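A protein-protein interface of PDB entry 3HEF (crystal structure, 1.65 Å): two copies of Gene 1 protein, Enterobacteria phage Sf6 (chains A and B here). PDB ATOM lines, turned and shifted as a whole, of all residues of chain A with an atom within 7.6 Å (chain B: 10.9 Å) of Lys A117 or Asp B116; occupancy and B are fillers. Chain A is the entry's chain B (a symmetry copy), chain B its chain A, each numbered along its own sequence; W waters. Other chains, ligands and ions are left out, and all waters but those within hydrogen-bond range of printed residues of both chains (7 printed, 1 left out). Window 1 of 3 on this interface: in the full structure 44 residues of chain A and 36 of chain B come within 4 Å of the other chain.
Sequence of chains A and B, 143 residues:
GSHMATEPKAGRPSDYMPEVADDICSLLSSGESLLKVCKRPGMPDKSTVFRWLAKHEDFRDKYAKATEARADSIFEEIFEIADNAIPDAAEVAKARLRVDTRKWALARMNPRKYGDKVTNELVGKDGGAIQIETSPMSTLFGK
The backbone carbonyl oxygen (O) of Lys A117 lies within hydrogen-bond range of the backbone NH (N) of Asp B116. The side-chain amide oxygen of Asn A120 lies close to the side-chain amide oxygen of Asn B120 (3.0 Å). The guanidinium group of Arg B108 is in hydrogen-bond range of the backbone carbonyl oxygen of Tyr A114 (2.9 Å). The backbone carbonyl oxygen (O) of Gly A115 lies within hydrogen-bond range of the guanidinium group (NH2) of Arg B108 (3.4 Å). The backbone carbonyl oxygen (O) of Asp B116 sits at hydrogen-bond distance from the backbone NH (N) of Thr A119 (2.9 Å). The backbone NH (N) of Val B118 lies within hydrogen-bond range of the backbone carbonyl oxygen (O) of Thr A119 (3.0 Å). NH2 of Arg B108 is in salt-bridge range of OD1 of Asp A116 (2.9 Å).
The backbone carbonyl oxygen (O) of Arg A112 sits at hydrogen-bond distance from the side-chain amino group (NZ) of Lys A117, at 2.9 Å. OD1 of Asn A110 is in hydrogen-bond range of N of Lys A113, at 3.2 Å. O of Lys A113 lies within hydrogen-bond range of NZ of Lys A117, at 3.3 Å. The side-chain amino group (NZ) of Lys B117 sits at hydrogen-bond distance from the backbone carbonyl oxygen (O) of Arg B112. O of Trp B104 is in hydrogen-bond range of NH1 of Arg B108 (3.0 Å).
CG of Arg B108 touches O of Lys A113, 3.4 Å away. Ala B107 touches Lys A117. CE of Lys A117 touches CG of Pro B111, 3.8 Å away. Lys A117 touches Gly B115. Asp B116 touches Val A118. CG1 of Val A118 touches CG2 of Val B118 (3.97 Å). Lys B117 touches Thr A119 (CA to O, 3.8 Å). Asn A120 touches Val B118 (CA to O, 3.3 Å).
Lys A117 touches four residues of chain B. Printed residues of chain A within 4 Å of Asp B116: Lys A117, Val A118 and Thr A119. Gly A115 touches one residue of chain B. Asp A116 touches just one residue of chain B: Arg B108 (2.9 Å). Of chain B, only Asp B116 and Val B118 come within 4 Å of Val A118. Thr A119 touches three residues of chain B. Of the printed residues of chain A, Ala B107 touches Lys A117 (3.4 Å). Of the printed residues of chain A, Pro B111 touches Lys A117 (3.8 Å). Printed residues of chain B within 4 Å of Tyr A114: Arg B108. Of the printed residues of chain A, Asn B120 touches Asn A120 (3.0 Å). Of the printed residues of chain A, Val B118 touches Val A118 (3.97 Å), Thr A119 (3.0 Å) and Asn A120 (3.3 Å). Met B109 touches none of the printed residues of chain A. The nearest residue of chain B that does not touch Lys A117 is Arg B108 (4.3 Å).
Of the 20 printed residues of chain B, 8 touch a printed residue of chain A. Printed residues of chain B that touch a printed residue of chain A: Ala B107, Arg B108, Pro B111, Gly B115, Asp B116, Lys B117, Val B118 and Asn B120. Hydrophobic or aromatic side chains of chain B within 4 Å of the printed part of chain A: Pro B111 and Val B118. Along chain B the printed residues that touch a printed residue of chain A span positions 107 to 120. Of the 11 printed residues of chain A, 8 touch a printed residue of chain B. Among the printed residues, 15 pairs touch across the chains.
Lys A117 touches Pro B111, but with the chains exchanged Pro A111 does not touch Lys B117 (16.2 Å). Lys A117 touches Gly B115, but with the chains exchanged Gly A115 does not touch Lys B117 (12.1 Å). Thr A119 touches Asp B116, but with the chains exchanged Asp A116 does not touch Thr B119 (14.6 Å). Thr A119 touches Val B118, but with the chains exchanged Val A118 does not touch Thr B119 (7.4 Å). Positions printed for both chains: 110, 111, 112, 113, 114, 115, 116, 117, 118, 119 and 120. Of the 15 pairs that touch across the chains among the printed residues, 2 have their exchanged pair printed and touching as well.
Water W5 lies within hydrogen-bond range of OD1 of Asp A116 (2.7 Å) and NE1 of Trp B104 (3.1 Å). Water W1 bridges O of Lys A113 (2.7 Å) and O of Arg B108 (2.8 Å). Water W3 bridges O of Arg B112 (2.8 Å) and OG1 of Thr A119 (3.1 Å). Water W7 bridges NH1 of Arg B108 (2.8 Å) and OD1 of Asp A116 (3.5 Å). Water W2 lies within hydrogen-bond range of OD1 of Asp A116 (2.9 Å) and NH2 of Arg B108 (3.3 Å). Water W4 lies within hydrogen-bond range of the backbone carbonyl oxygen of Thr A119 and the backbone carbonyl oxygen of Val B118.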
ATOM      1  N   ASN A 110     -29.804 -38.576 -36.686  1.00  0.00           N
ATOM      2  CA  ASN A 110     -30.367 -38.580 -35.324  1.00  0.00           C
ATOM      3  C   ASN A 110     -30.368 -37.125 -34.851  1.00  0.00           C
ATOM      4  O   ASN A 110     -29.467 -36.690 -34.129  1.00  0.00           O
ATOM      5  CB  ASN A 110     -29.531 -39.448 -34.373  1.00  0.00           C
ATOM      6  CG  ASN A 110     -30.234 -39.681 -33.049  1.00  0.00           C
ATOM      7  OD1 ASN A 110     -31.079 -38.867 -32.632  1.00  0.00           O
ATOM      8  ND2 ASN A 110     -29.871 -40.766 -32.358  1.00  0.00           N
ATOM      9  N   PRO A 111     -31.385 -36.354 -35.268  1.00  0.00           N
ATOM     10  CA  PRO A 111     -31.477 -34.936 -34.887  1.00  0.00           C
ATOM     11  C   PRO A 111     -31.456 -34.668 -33.411  1.00  0.00           C
ATOM     12  O   PRO A 111     -30.799 -33.727 -32.943  1.00  0.00           O
ATOM     13  CB  PRO A 111     -32.796 -34.465 -35.512  1.00  0.00           C
ATOM     14  CG  PRO A 111     -33.066 -35.424 -36.595  1.00  0.00           C
ATOM     15  CD  PRO A 111     -32.533 -36.758 -36.098  1.00  0.00           C
ATOM     16  N   ARG A 112     -32.177 -35.484 -32.648  1.00  0.00           N
ATOM     17  CA  ARG A 112     -32.231 -35.283 -31.207  1.00  0.00           C
ATOM     18  C   ARG A 112     -30.862 -35.349 -30.552  1.00  0.00           C
ATOM     19  O   ARG A 112     -30.514 -34.524 -29.690  1.00  0.00           O
ATOM     20  CB  ARG A 112     -33.141 -36.342 -30.575  1.00  0.00           C
ATOM     21  CG  ARG A 112     -33.355 -36.195 -29.090  1.00  0.00           C
ATOM     22  CD  ARG A 112     -34.588 -36.999 -28.649  1.00  0.00           C
ATOM     23  NE  ARG A 112     -34.333 -38.430 -28.478  1.00  0.00           N
ATOM     24  CZ  ARG A 112     -35.279 -39.367 -28.567  1.00  0.00           C
ATOM     25  NH1 ARG A 112     -36.542 -39.022 -28.836  1.00  0.00           N
ATOM     26  NH2 ARG A 112     -34.970 -40.648 -28.373  1.00  0.00           N
ATOM     27  N   LYS A 113     -30.068 -36.325 -30.973  1.00  0.00           N
ATOM     28  CA  LYS A 113     -28.758 -36.508 -30.389  1.00  0.00           C
ATOM     29  C   LYS A 113     -27.671 -35.648 -30.999  1.00  0.00           C
ATOM     30  O   LYS A 113     -26.861 -35.063 -30.285  1.00  0.00           O
ATOM     31  CB  LYS A 113     -28.358 -37.964 -30.545  1.00  0.00           C
ATOM     32  CG  LYS A 113     -27.132 -38.338 -29.774  1.00  0.00           C
ATOM     33  CD  LYS A 113     -27.094 -39.851 -29.610  1.00  0.00           C
ATOM     34  CE  LYS A 113     -25.851 -40.269 -28.886  1.00  0.00           C
ATOM     35  NZ  LYS A 113     -25.743 -41.767 -28.852  1.00  0.00           N
ATOM     36  N   TYR A 114     -27.672 -35.570 -32.325  1.00  0.00           N
ATOM     37  CA  TYR A 114     -26.600 -34.880 -33.020  1.00  0.00           C
ATOM     38  C   TYR A 114     -26.870 -33.521 -33.647  1.00  0.00           C
ATOM     39  O   TYR A 114     -25.984 -32.970 -34.311  1.00  0.00           O
ATOM     40  CB  TYR A 114     -25.990 -35.844 -34.073  1.00  0.00           C
ATOM     41  CG  TYR A 114     -25.439 -37.109 -33.471  1.00  0.00           C
ATOM     42  CD1 TYR A 114     -24.419 -37.060 -32.516  1.00  0.00           C
ATOM     43  CD2 TYR A 114     -25.947 -38.352 -33.837  1.00  0.00           C
ATOM     44  CE1 TYR A 114     -23.922 -38.220 -31.925  1.00  0.00           C
ATOM     45  CE2 TYR A 114     -25.447 -39.536 -33.255  1.00  0.00           C
ATOM     46  CZ  TYR A 114     -24.440 -39.441 -32.303  1.00  0.00           C
ATOM     47  OH  TYR A 114     -23.921 -40.558 -31.695  1.00  0.00           O
ATOM     48  N   GLY A 115     -28.077 -32.967 -33.466  1.00  0.00           N
ATOM     49  CA  GLY A 115     -28.328 -31.626 -33.985  1.00  0.00           C
ATOM     50  C   GLY A 115     -27.529 -30.607 -33.166  1.00  0.00           C
ATOM     51  O   GLY A 115     -26.943 -30.919 -32.122  1.00  0.00           O
ATOM     52  N   ASP A 116     -27.529 -29.362 -33.633  1.00  0.00           N
ATOM     53  CA  ASP A 116     -26.843 -28.289 -32.948  1.00  0.00           C
ATOM     54  C   ASP A 116     -27.474 -28.071 -31.574  1.00  0.00           C
ATOM     55  O   ASP A 116     -28.651 -28.363 -31.382  1.00  0.00           O
ATOM     56  CB  ASP A 116     -26.956 -27.002 -33.763  1.00  0.00           C
ATOM     57  CG  ASP A 116     -25.941 -26.924 -34.903  1.00  0.00           C
ATOM     58  OD1 ASP A 116     -25.083 -27.844 -35.059  1.00  0.00           O
ATOM     59  OD2 ASP A 116     -26.029 -25.911 -35.638  1.00  0.00           O
ATOM     60  N   LYS A 117     -26.685 -27.538 -30.648  1.00  0.00           N
ATOM     61  CA  LYS A 117     -27.121 -27.304 -29.281  1.00  0.00           C
ATOM     62  C   LYS A 117     -26.882 -25.830 -28.939  1.00  0.00           C
ATOM     63  O   LYS A 117     -25.754 -25.355 -29.013  1.00  0.00           O
ATOM     64  CB  LYS A 117     -26.306 -28.173 -28.316  1.00  0.00           C
ATOM     65  CG  LYS A 117     -26.197 -29.637 -28.716  1.00  0.00           C
ATOM     66  CD  LYS A 117     -27.542 -30.276 -28.757  1.00  0.00           C
ATOM     67  CE  LYS A 117     -27.336 -31.777 -28.964  1.00  0.00           C
ATOM     68  NZ  LYS A 117     -28.582 -32.417 -29.337  1.00  0.00           N
ATOM     69  N   VAL A 118     -27.928 -25.095 -28.547  1.00  0.00           N
ATOM     70  CA  VAL A 118     -27.732 -23.694 -28.215  1.00  0.00           C
ATOM     71  C   VAL A 118     -28.544 -23.401 -26.967  1.00  0.00           C
ATOM     72  O   VAL A 118     -29.619 -23.969 -26.825  1.00  0.00           O
ATOM     73  CB  VAL A 118     -28.304 -22.751 -29.305  1.00  0.00           C
ATOM     74  CG1 VAL A 118     -28.036 -21.306 -28.933  1.00  0.00           C
ATOM     75  CG2 VAL A 118     -27.705 -23.069 -30.673  1.00  0.00           C
ATOM     76  N   THR A 119     -27.989 -22.586 -26.087  1.00  0.00           N
ATOM     77  CA  THR A 119     -28.758 -22.124 -24.918  1.00  0.00           C
ATOM     78  C   THR A 119     -28.934 -20.622 -25.184  1.00  0.00           C
ATOM     79  O   THR A 119     -27.958 -19.883 -25.335  1.00  0.00           O
ATOM     80  CB  THR A 119     -28.001 -22.324 -23.617  1.00  0.00           C
ATOM     81  OG1 THR A 119     -27.822 -23.729 -23.409  1.00  0.00           O
ATOM     82  CG2 THR A 119     -28.791 -21.700 -22.464  1.00  0.00           C
ATOM     83  N   ASN A 120     -30.181 -20.152 -25.256  1.00  0.00           N
ATOM     84  CA  ASN A 120     -30.427 -18.734 -25.518  1.00  0.00           C
ATOM     85  C   ASN A 120     -30.953 -18.093 -24.248  1.00  0.00           C
ATOM     86  O   ASN A 120     -32.011 -18.499 -23.781  1.00  0.00           O
ATOM     87  CB  ASN A 120     -31.514 -18.563 -26.586  1.00  0.00           C
ATOM     88  CG  ASN A 120     -31.105 -19.095 -27.952  1.00  0.00           C
ATOM     89  OD1 ASN A 120     -30.521 -18.356 -28.782  1.00  0.00           O
ATOM     90  ND2 ASN A 120     -31.425 -20.343 -28.202  1.00  0.00           N
ATOM     91  N   ASP B 100     -11.520 -28.579 -34.186  1.00  0.00           N
ATOM     92  CA  ASP B 100     -12.913 -28.347 -34.629  1.00  0.00           C
ATOM     93  C   ASP B 100     -13.789 -29.575 -34.427  1.00  0.00           C
ATOM     94  O   ASP B 100     -14.983 -29.470 -34.080  1.00  0.00           O
ATOM     95  CB  ASP B 100     -12.926 -27.917 -36.107  1.00  0.00           C
ATOM     96  CG  ASP B 100     -12.435 -26.485 -36.308  1.00  0.00           C
ATOM     97  OD1 ASP B 100     -12.277 -25.726 -35.318  1.00  0.00           O
ATOM     98  OD2 ASP B 100     -12.217 -26.107 -37.482  1.00  0.00           O
ATOM     99  N   ARG B 102     -13.406 -31.914 -32.141  1.00  0.00           N
ATOM    100  CA  ARG B 102     -13.653 -32.020 -30.711  1.00  0.00           C
ATOM    101  C   ARG B 102     -14.664 -30.980 -30.230  1.00  0.00           C
ATOM    102  O   ARG B 102     -15.527 -31.320 -29.402  1.00  0.00           O
ATOM    103  CB  ARG B 102     -12.336 -31.874 -29.951  1.00  0.00           C
ATOM    104  CG  ARG B 102     -11.493 -33.171 -30.001  1.00  0.00           C
ATOM    105  CD  ARG B 102     -10.046 -32.925 -29.574  1.00  0.00           C
ATOM    106  NE  ARG B 102      -9.291 -34.176 -29.480  1.00  0.00           N
ATOM    107  CZ  ARG B 102      -8.866 -34.903 -30.518  1.00  0.00           C
ATOM    108  NH1 ARG B 102      -9.105 -34.539 -31.774  1.00  0.00           N
ATOM    109  NH2 ARG B 102      -8.158 -36.005 -30.281  1.00  0.00           N
ATOM    110  N   LYS B 103     -14.562 -29.744 -30.717  1.00  0.00           N
ATOM    111  CA  LYS B 103     -15.526 -28.709 -30.272  1.00  0.00           C
ATOM    112  C   LYS B 103     -16.937 -29.138 -30.623  1.00  0.00           C
ATOM    113  O   LYS B 103     -17.877 -29.038 -29.795  1.00  0.00           O
ATOM    114  CB  LYS B 103     -15.238 -27.351 -30.921  1.00  0.00           C
ATOM    115  CG  LYS B 103     -13.966 -26.705 -30.379  1.00  0.00           C
ATOM    116  CD  LYS B 103     -13.680 -25.323 -30.966  1.00  0.00           C
ATOM    117  CE  LYS B 103     -13.882 -25.238 -32.438  1.00  0.00           C
ATOM    118  NZ  LYS B 103     -13.501 -23.886 -32.976  1.00  0.00           N
ATOM    119  N   TRP B 104     -17.110 -29.582 -31.863  1.00  0.00           N
ATOM    120  CA  TRP B 104     -18.420 -30.016 -32.346  1.00  0.00           C
ATOM    121  C   TRP B 104     -18.920 -31.191 -31.520  1.00  0.00           C
ATOM    122  O   TRP B 104     -20.070 -31.210 -31.080  1.00  0.00           O
ATOM    123  CB  TRP B 104     -18.302 -30.432 -33.814  1.00  0.00           C
ATOM    124  CG  TRP B 104     -19.590 -30.735 -34.478  1.00  0.00           C
ATOM    125  CD1 TRP B 104     -20.383 -29.862 -35.179  1.00  0.00           C
ATOM    126  CD2 TRP B 104     -20.198 -32.017 -34.587  1.00  0.00           C
ATOM    127  NE1 TRP B 104     -21.457 -30.538 -35.730  1.00  0.00           N
ATOM    128  CE2 TRP B 104     -21.374 -31.860 -35.382  1.00  0.00           C
ATOM    129  CE3 TRP B 104     -19.873 -33.288 -34.103  1.00  0.00           C
ATOM    130  CZ2 TRP B 104     -22.216 -32.932 -35.700  1.00  0.00           C
ATOM    131  CZ3 TRP B 104     -20.730 -34.383 -34.436  1.00  0.00           C
ATOM    132  CH2 TRP B 104     -21.879 -34.175 -35.227  1.00  0.00           C
ATOM    133  N   ALA B 105     -18.058 -32.164 -31.280  1.00  0.00           N
ATOM    134  CA  ALA B 105     -18.445 -33.329 -30.510  1.00  0.00           C
ATOM    135  C   ALA B 105     -18.792 -33.017 -29.047  1.00  0.00           C
ATOM    136  O   ALA B 105     -19.704 -33.647 -28.504  1.00  0.00           O
ATOM    137  CB  ALA B 105     -17.328 -34.369 -30.563  1.00  0.00           C
ATOM    138  N   LEU B 106     -18.064 -32.088 -28.427  1.00  0.00           N
ATOM    139  CA  LEU B 106     -18.308 -31.748 -27.001  1.00  0.00           C
ATOM    140  C   LEU B 106     -19.724 -31.257 -26.810  1.00  0.00           C
ATOM    141  O   LEU B 106     -20.360 -31.565 -25.794  1.00  0.00           O
ATOM    142  CB  LEU B 106     -17.355 -30.641 -26.533  1.00  0.00           C
ATOM    143  CG  LEU B 106     -16.131 -31.112 -25.703  1.00  0.00           C
ATOM    144  CD1 LEU B 106     -15.646 -32.478 -26.114  1.00  0.00           C
ATOM    145  CD2 LEU B 106     -15.031 -30.020 -25.848  1.00  0.00           C
ATOM    146  N   ALA B 107     -20.209 -30.471 -27.758  1.00  0.00           N
ATOM    147  CA  ALA B 107     -21.578 -29.951 -27.612  1.00  0.00           C
ATOM    148  C   ALA B 107     -22.572 -31.102 -27.585  1.00  0.00           C
ATOM    149  O   ALA B 107     -23.630 -31.002 -26.925  1.00  0.00           O
ATOM    150  CB  ALA B 107     -21.919 -29.001 -28.746  1.00  0.00           C
ATOM    151  N   ARG B 108     -22.275 -32.184 -28.308  1.00  0.00           N
ATOM    152  CA  ARG B 108     -23.184 -33.327 -28.301  1.00  0.00           C
ATOM    153  C   ARG B 108     -22.994 -34.241 -27.087  1.00  0.00           C
ATOM    154  O   ARG B 108     -23.939 -34.910 -26.656  1.00  0.00           O
ATOM    155  CB  ARG B 108     -23.049 -34.142 -29.577  1.00  0.00           C
ATOM    156  CG  ARG B 108     -23.817 -33.495 -30.698  1.00  0.00           C
ATOM    157  CD  ARG B 108     -22.893 -32.902 -31.709  1.00  0.00           C
ATOM    158  NE  ARG B 108     -23.641 -32.204 -32.751  1.00  0.00           N
ATOM    159  CZ  ARG B 108     -23.444 -30.939 -33.083  1.00  0.00           C
ATOM    160  NH1 ARG B 108     -22.518 -30.210 -32.469  1.00  0.00           N
ATOM    161  NH2 ARG B 108     -24.181 -30.402 -34.037  1.00  0.00           N
ATOM    162  N   MET B 109     -21.783 -34.291 -26.548  1.00  0.00           N
ATOM    163  CA  MET B 109     -21.533 -35.132 -25.377  1.00  0.00           C
ATOM    164  C   MET B 109     -22.155 -34.504 -24.124  1.00  0.00           C
ATOM    165  O   MET B 109     -22.636 -35.226 -23.244  1.00  0.00           O
ATOM    166  CB  MET B 109     -20.033 -35.345 -25.198  1.00  0.00           C
ATOM    167  CG  MET B 109     -19.465 -36.034 -26.395  1.00  0.00           C
ATOM    168  SD  MET B 109     -17.684 -36.124 -26.225  1.00  0.00           S
ATOM    169  CE  MET B 109     -17.255 -37.005 -27.604  1.00  0.00           C
ATOM    170  N   ASN B 110     -22.142 -33.176 -24.033  1.00  0.00           N
ATOM    171  CA  ASN B 110     -22.779 -32.507 -22.884  1.00  0.00           C
ATOM    172  C   ASN B 110     -23.370 -31.184 -23.387  1.00  0.00           C
ATOM    173  O   ASN B 110     -22.764 -30.116 -23.259  1.00  0.00           O
ATOM    174  CB  ASN B 110     -21.776 -32.273 -21.767  1.00  0.00           C
ATOM    175  CG  ASN B 110     -22.440 -31.824 -20.484  1.00  0.00           C
ATOM    176  OD1 ASN B 110     -23.574 -31.310 -20.505  1.00  0.00           O
ATOM    177  ND2 ASN B 110     -21.733 -31.972 -19.372  1.00  0.00           N
ATOM    178  N   PRO B 111     -24.574 -31.244 -23.958  1.00  0.00           N
ATOM    179  CA  PRO B 111     -25.224 -30.042 -24.493  1.00  0.00           C
ATOM    180  C   PRO B 111     -25.392 -28.863 -23.553  1.00  0.00           C
ATOM    181  O   PRO B 111     -25.136 -27.709 -23.922  1.00  0.00           O
ATOM    182  CB  PRO B 111     -26.575 -30.573 -25.013  1.00  0.00           C
ATOM    183  CG  PRO B 111     -26.270 -31.974 -25.370  1.00  0.00           C
ATOM    184  CD  PRO B 111     -25.379 -32.448 -24.254  1.00  0.00           C
ATOM    185  N   ARG B 112     -25.822 -29.133 -22.330  1.00  0.00           N
ATOM    186  CA  ARG B 112     -26.035 -28.045 -21.403  1.00  0.00           C
ATOM    187  C   ARG B 112     -24.745 -27.317 -21.093  1.00  0.00           C
ATOM    188  O   ARG B 112     -24.747 -26.083 -20.959  1.00  0.00           O
ATOM    189  CB  ARG B 112     -26.685 -28.589 -20.123  1.00  0.00           C
ATOM    190  CG  ARG B 112     -27.082 -27.544 -19.115  1.00  0.00           C
ATOM    191  CD  ARG B 112     -27.756 -28.214 -17.910  1.00  0.00           C
ATOM    192  NE  ARG B 112     -26.937 -29.303 -17.374  1.00  0.00           N
ATOM    193  CZ  ARG B 112     -27.249 -30.028 -16.302  1.00  0.00           C
ATOM    194  NH1 ARG B 112     -28.375 -29.785 -15.635  1.00  0.00           N
ATOM    195  NH2 ARG B 112     -26.435 -30.997 -15.895  1.00  0.00           N
ATOM    196  N   LYS B 113     -23.631 -28.059 -21.056  1.00  0.00           N
ATOM    197  CA  LYS B 113     -22.347 -27.476 -20.724  1.00  0.00           C
ATOM    198  C   LYS B 113     -21.549 -26.915 -21.895  1.00  0.00           C
ATOM    199  O   LYS B 113     -21.043 -25.787 -21.818  1.00  0.00           O
ATOM    200  CB  LYS B 113     -21.481 -28.513 -19.999  1.00  0.00           C
ATOM    201  CG  LYS B 113     -20.174 -27.990 -19.488  1.00  0.00           C
ATOM    202  CD  LYS B 113     -19.563 -28.918 -18.439  1.00  0.00           C
ATOM    203  CE  LYS B 113     -18.366 -28.240 -17.792  1.00  0.00           C
ATOM    204  NZ  LYS B 113     -17.571 -29.221 -17.011  1.00  0.00           N
ATOM    205  N   TYR B 114     -21.470 -27.680 -22.980  1.00  0.00           N
ATOM    206  CA  TYR B 114     -20.642 -27.291 -24.119  1.00  0.00           C
ATOM    207  C   TYR B 114     -21.380 -26.805 -25.358  1.00  0.00           C
ATOM    208  O   TYR B 114     -20.763 -26.571 -26.393  1.00  0.00           O
ATOM    209  CB  TYR B 114     -19.705 -28.464 -24.496  1.00  0.00           C
ATOM    210  CG  TYR B 114     -18.741 -28.797 -23.386  1.00  0.00           C
ATOM    211  CD1 TYR B 114     -17.863 -27.822 -22.886  1.00  0.00           C
ATOM    212  CD2 TYR B 114     -18.743 -30.065 -22.786  1.00  0.00           C
ATOM    213  CE1 TYR B 114     -17.009 -28.099 -21.814  1.00  0.00           C
ATOM    214  CE2 TYR B 114     -17.878 -30.350 -21.693  1.00  0.00           C
ATOM    215  CZ  TYR B 114     -17.032 -29.358 -21.234  1.00  0.00           C
ATOM    216  OH  TYR B 114     -16.190 -29.588 -20.169  1.00  0.00           O
ATOM    217  N   GLY B 115     -22.702 -26.664 -25.279  1.00  0.00           N
ATOM    218  CA  GLY B 115     -23.421 -26.155 -26.440  1.00  0.00           C
ATOM    219  C   GLY B 115     -23.132 -24.657 -26.585  1.00  0.00           C
ATOM    220  O   GLY B 115     -22.497 -24.050 -25.725  1.00  0.00           O
ATOM    221  N   ASP B 116     -23.620 -24.066 -27.669  1.00  0.00           N
ATOM    222  CA  ASP B 116     -23.437 -22.648 -27.957  1.00  0.00           C
ATOM    223  C   ASP B 116     -24.141 -21.814 -26.901  1.00  0.00           C
ATOM    224  O   ASP B 116     -25.132 -22.259 -26.331  1.00  0.00           O
ATOM    225  CB  ASP B 116     -24.015 -22.307 -29.340  1.00  0.00           C
ATOM    226  CG  ASP B 116     -23.045 -22.594 -30.486  1.00  0.00           C
ATOM    227  OD1 ASP B 116     -21.913 -23.068 -30.227  1.00  0.00           O
ATOM    228  OD2 ASP B 116     -23.441 -22.325 -31.645  1.00  0.00           O
ATOM    229  N   LYS B 117     -23.649 -20.604 -26.687  1.00  0.00           N
ATOM    230  CA  LYS B 117     -24.180 -19.710 -25.671  1.00  0.00           C
ATOM    231  C   LYS B 117     -24.521 -18.398 -26.321  1.00  0.00           C
ATOM    232  O   LYS B 117     -23.643 -17.748 -26.905  1.00  0.00           O
ATOM    233  CB  LYS B 117     -23.120 -19.489 -24.584  1.00  0.00           C
ATOM    234  CG  LYS B 117     -22.489 -20.776 -24.053  1.00  0.00           C
ATOM    235  CD  LYS B 117     -23.542 -21.630 -23.367  1.00  0.00           C
ATOM    236  CE  LYS B 117     -22.878 -22.907 -22.860  1.00  0.00           C
ATOM    237  NZ  LYS B 117     -23.865 -23.696 -22.101  1.00  0.00           N
ATOM    238  N   VAL B 118     -25.781 -17.970 -26.238  1.00  0.00           N
ATOM    239  CA  VAL B 118     -26.159 -16.710 -26.838  1.00  0.00           C
ATOM    240  C   VAL B 118     -27.098 -15.961 -25.888  1.00  0.00           C
ATOM    241  O   VAL B 118     -27.889 -16.595 -25.208  1.00  0.00           O
ATOM    242  CB  VAL B 118     -26.962 -16.915 -28.166  1.00  0.00           C
ATOM    243  CG1 VAL B 118     -27.257 -15.555 -28.796  1.00  0.00           C
ATOM    244  CG2 VAL B 118     -26.170 -17.811 -29.170  1.00  0.00           C
ATOM    245  N   THR B 119     -26.932 -14.650 -25.802  1.00  0.00           N
ATOM    246  CA  THR B 119     -27.875 -13.844 -25.033  1.00  0.00           C
ATOM    247  C   THR B 119     -28.557 -12.993 -26.100  1.00  0.00           C
ATOM    248  O   THR B 119     -27.902 -12.236 -26.832  1.00  0.00           O
ATOM    249  CB  THR B 119     -27.159 -12.938 -24.034  1.00  0.00           C
ATOM    250  OG1 THR B 119     -26.459 -13.757 -23.084  1.00  0.00           O
ATOM    251  CG2 THR B 119     -28.186 -12.007 -23.330  1.00  0.00           C
ATOM    252  N   ASN B 120     -29.881 -13.092 -26.196  1.00  0.00           N
ATOM    253  CA  ASN B 120     -30.630 -12.340 -27.186  1.00  0.00           C
ATOM    254  C   ASN B 120     -31.434 -11.269 -26.504  1.00  0.00           C
ATOM    255  O   ASN B 120     -32.269 -11.615 -25.681  1.00  0.00           O
ATOM    256  CB  ASN B 120     -31.649 -13.236 -27.933  1.00  0.00           C
ATOM    257  CG  ASN B 120     -30.998 -14.381 -28.685  1.00  0.00           C
ATOM    258  OD1 ASN B 120     -30.783 -15.477 -28.128  1.00  0.00           O
ATOM    259  ND2 ASN B 120     -30.712 -14.136 -29.975  1.00  0.00           N
HETATM  260  O   HOH W   1     -26.567 -34.985 -27.611  1.00  0.00           O
HETATM  261  O   HOH W   2     -26.193 -30.021 -36.664  1.00  0.00           O
HETATM  262  O   HOH W   3     -27.048 -24.505 -20.493  1.00  0.00           O
HETATM  263  O   HOH W   4     -26.428 -18.729 -22.948  1.00  0.00           O
HETATM  264  O   HOH W   5     -23.011 -28.019 -36.707  1.00  0.00           O
HETATM  265  O   HOH W   6     -27.649 -26.349 -24.891  1.00  0.00           O
HETATM  266  O   HOH W   7     -22.118 -27.506 -33.240  1.00  0.00           O
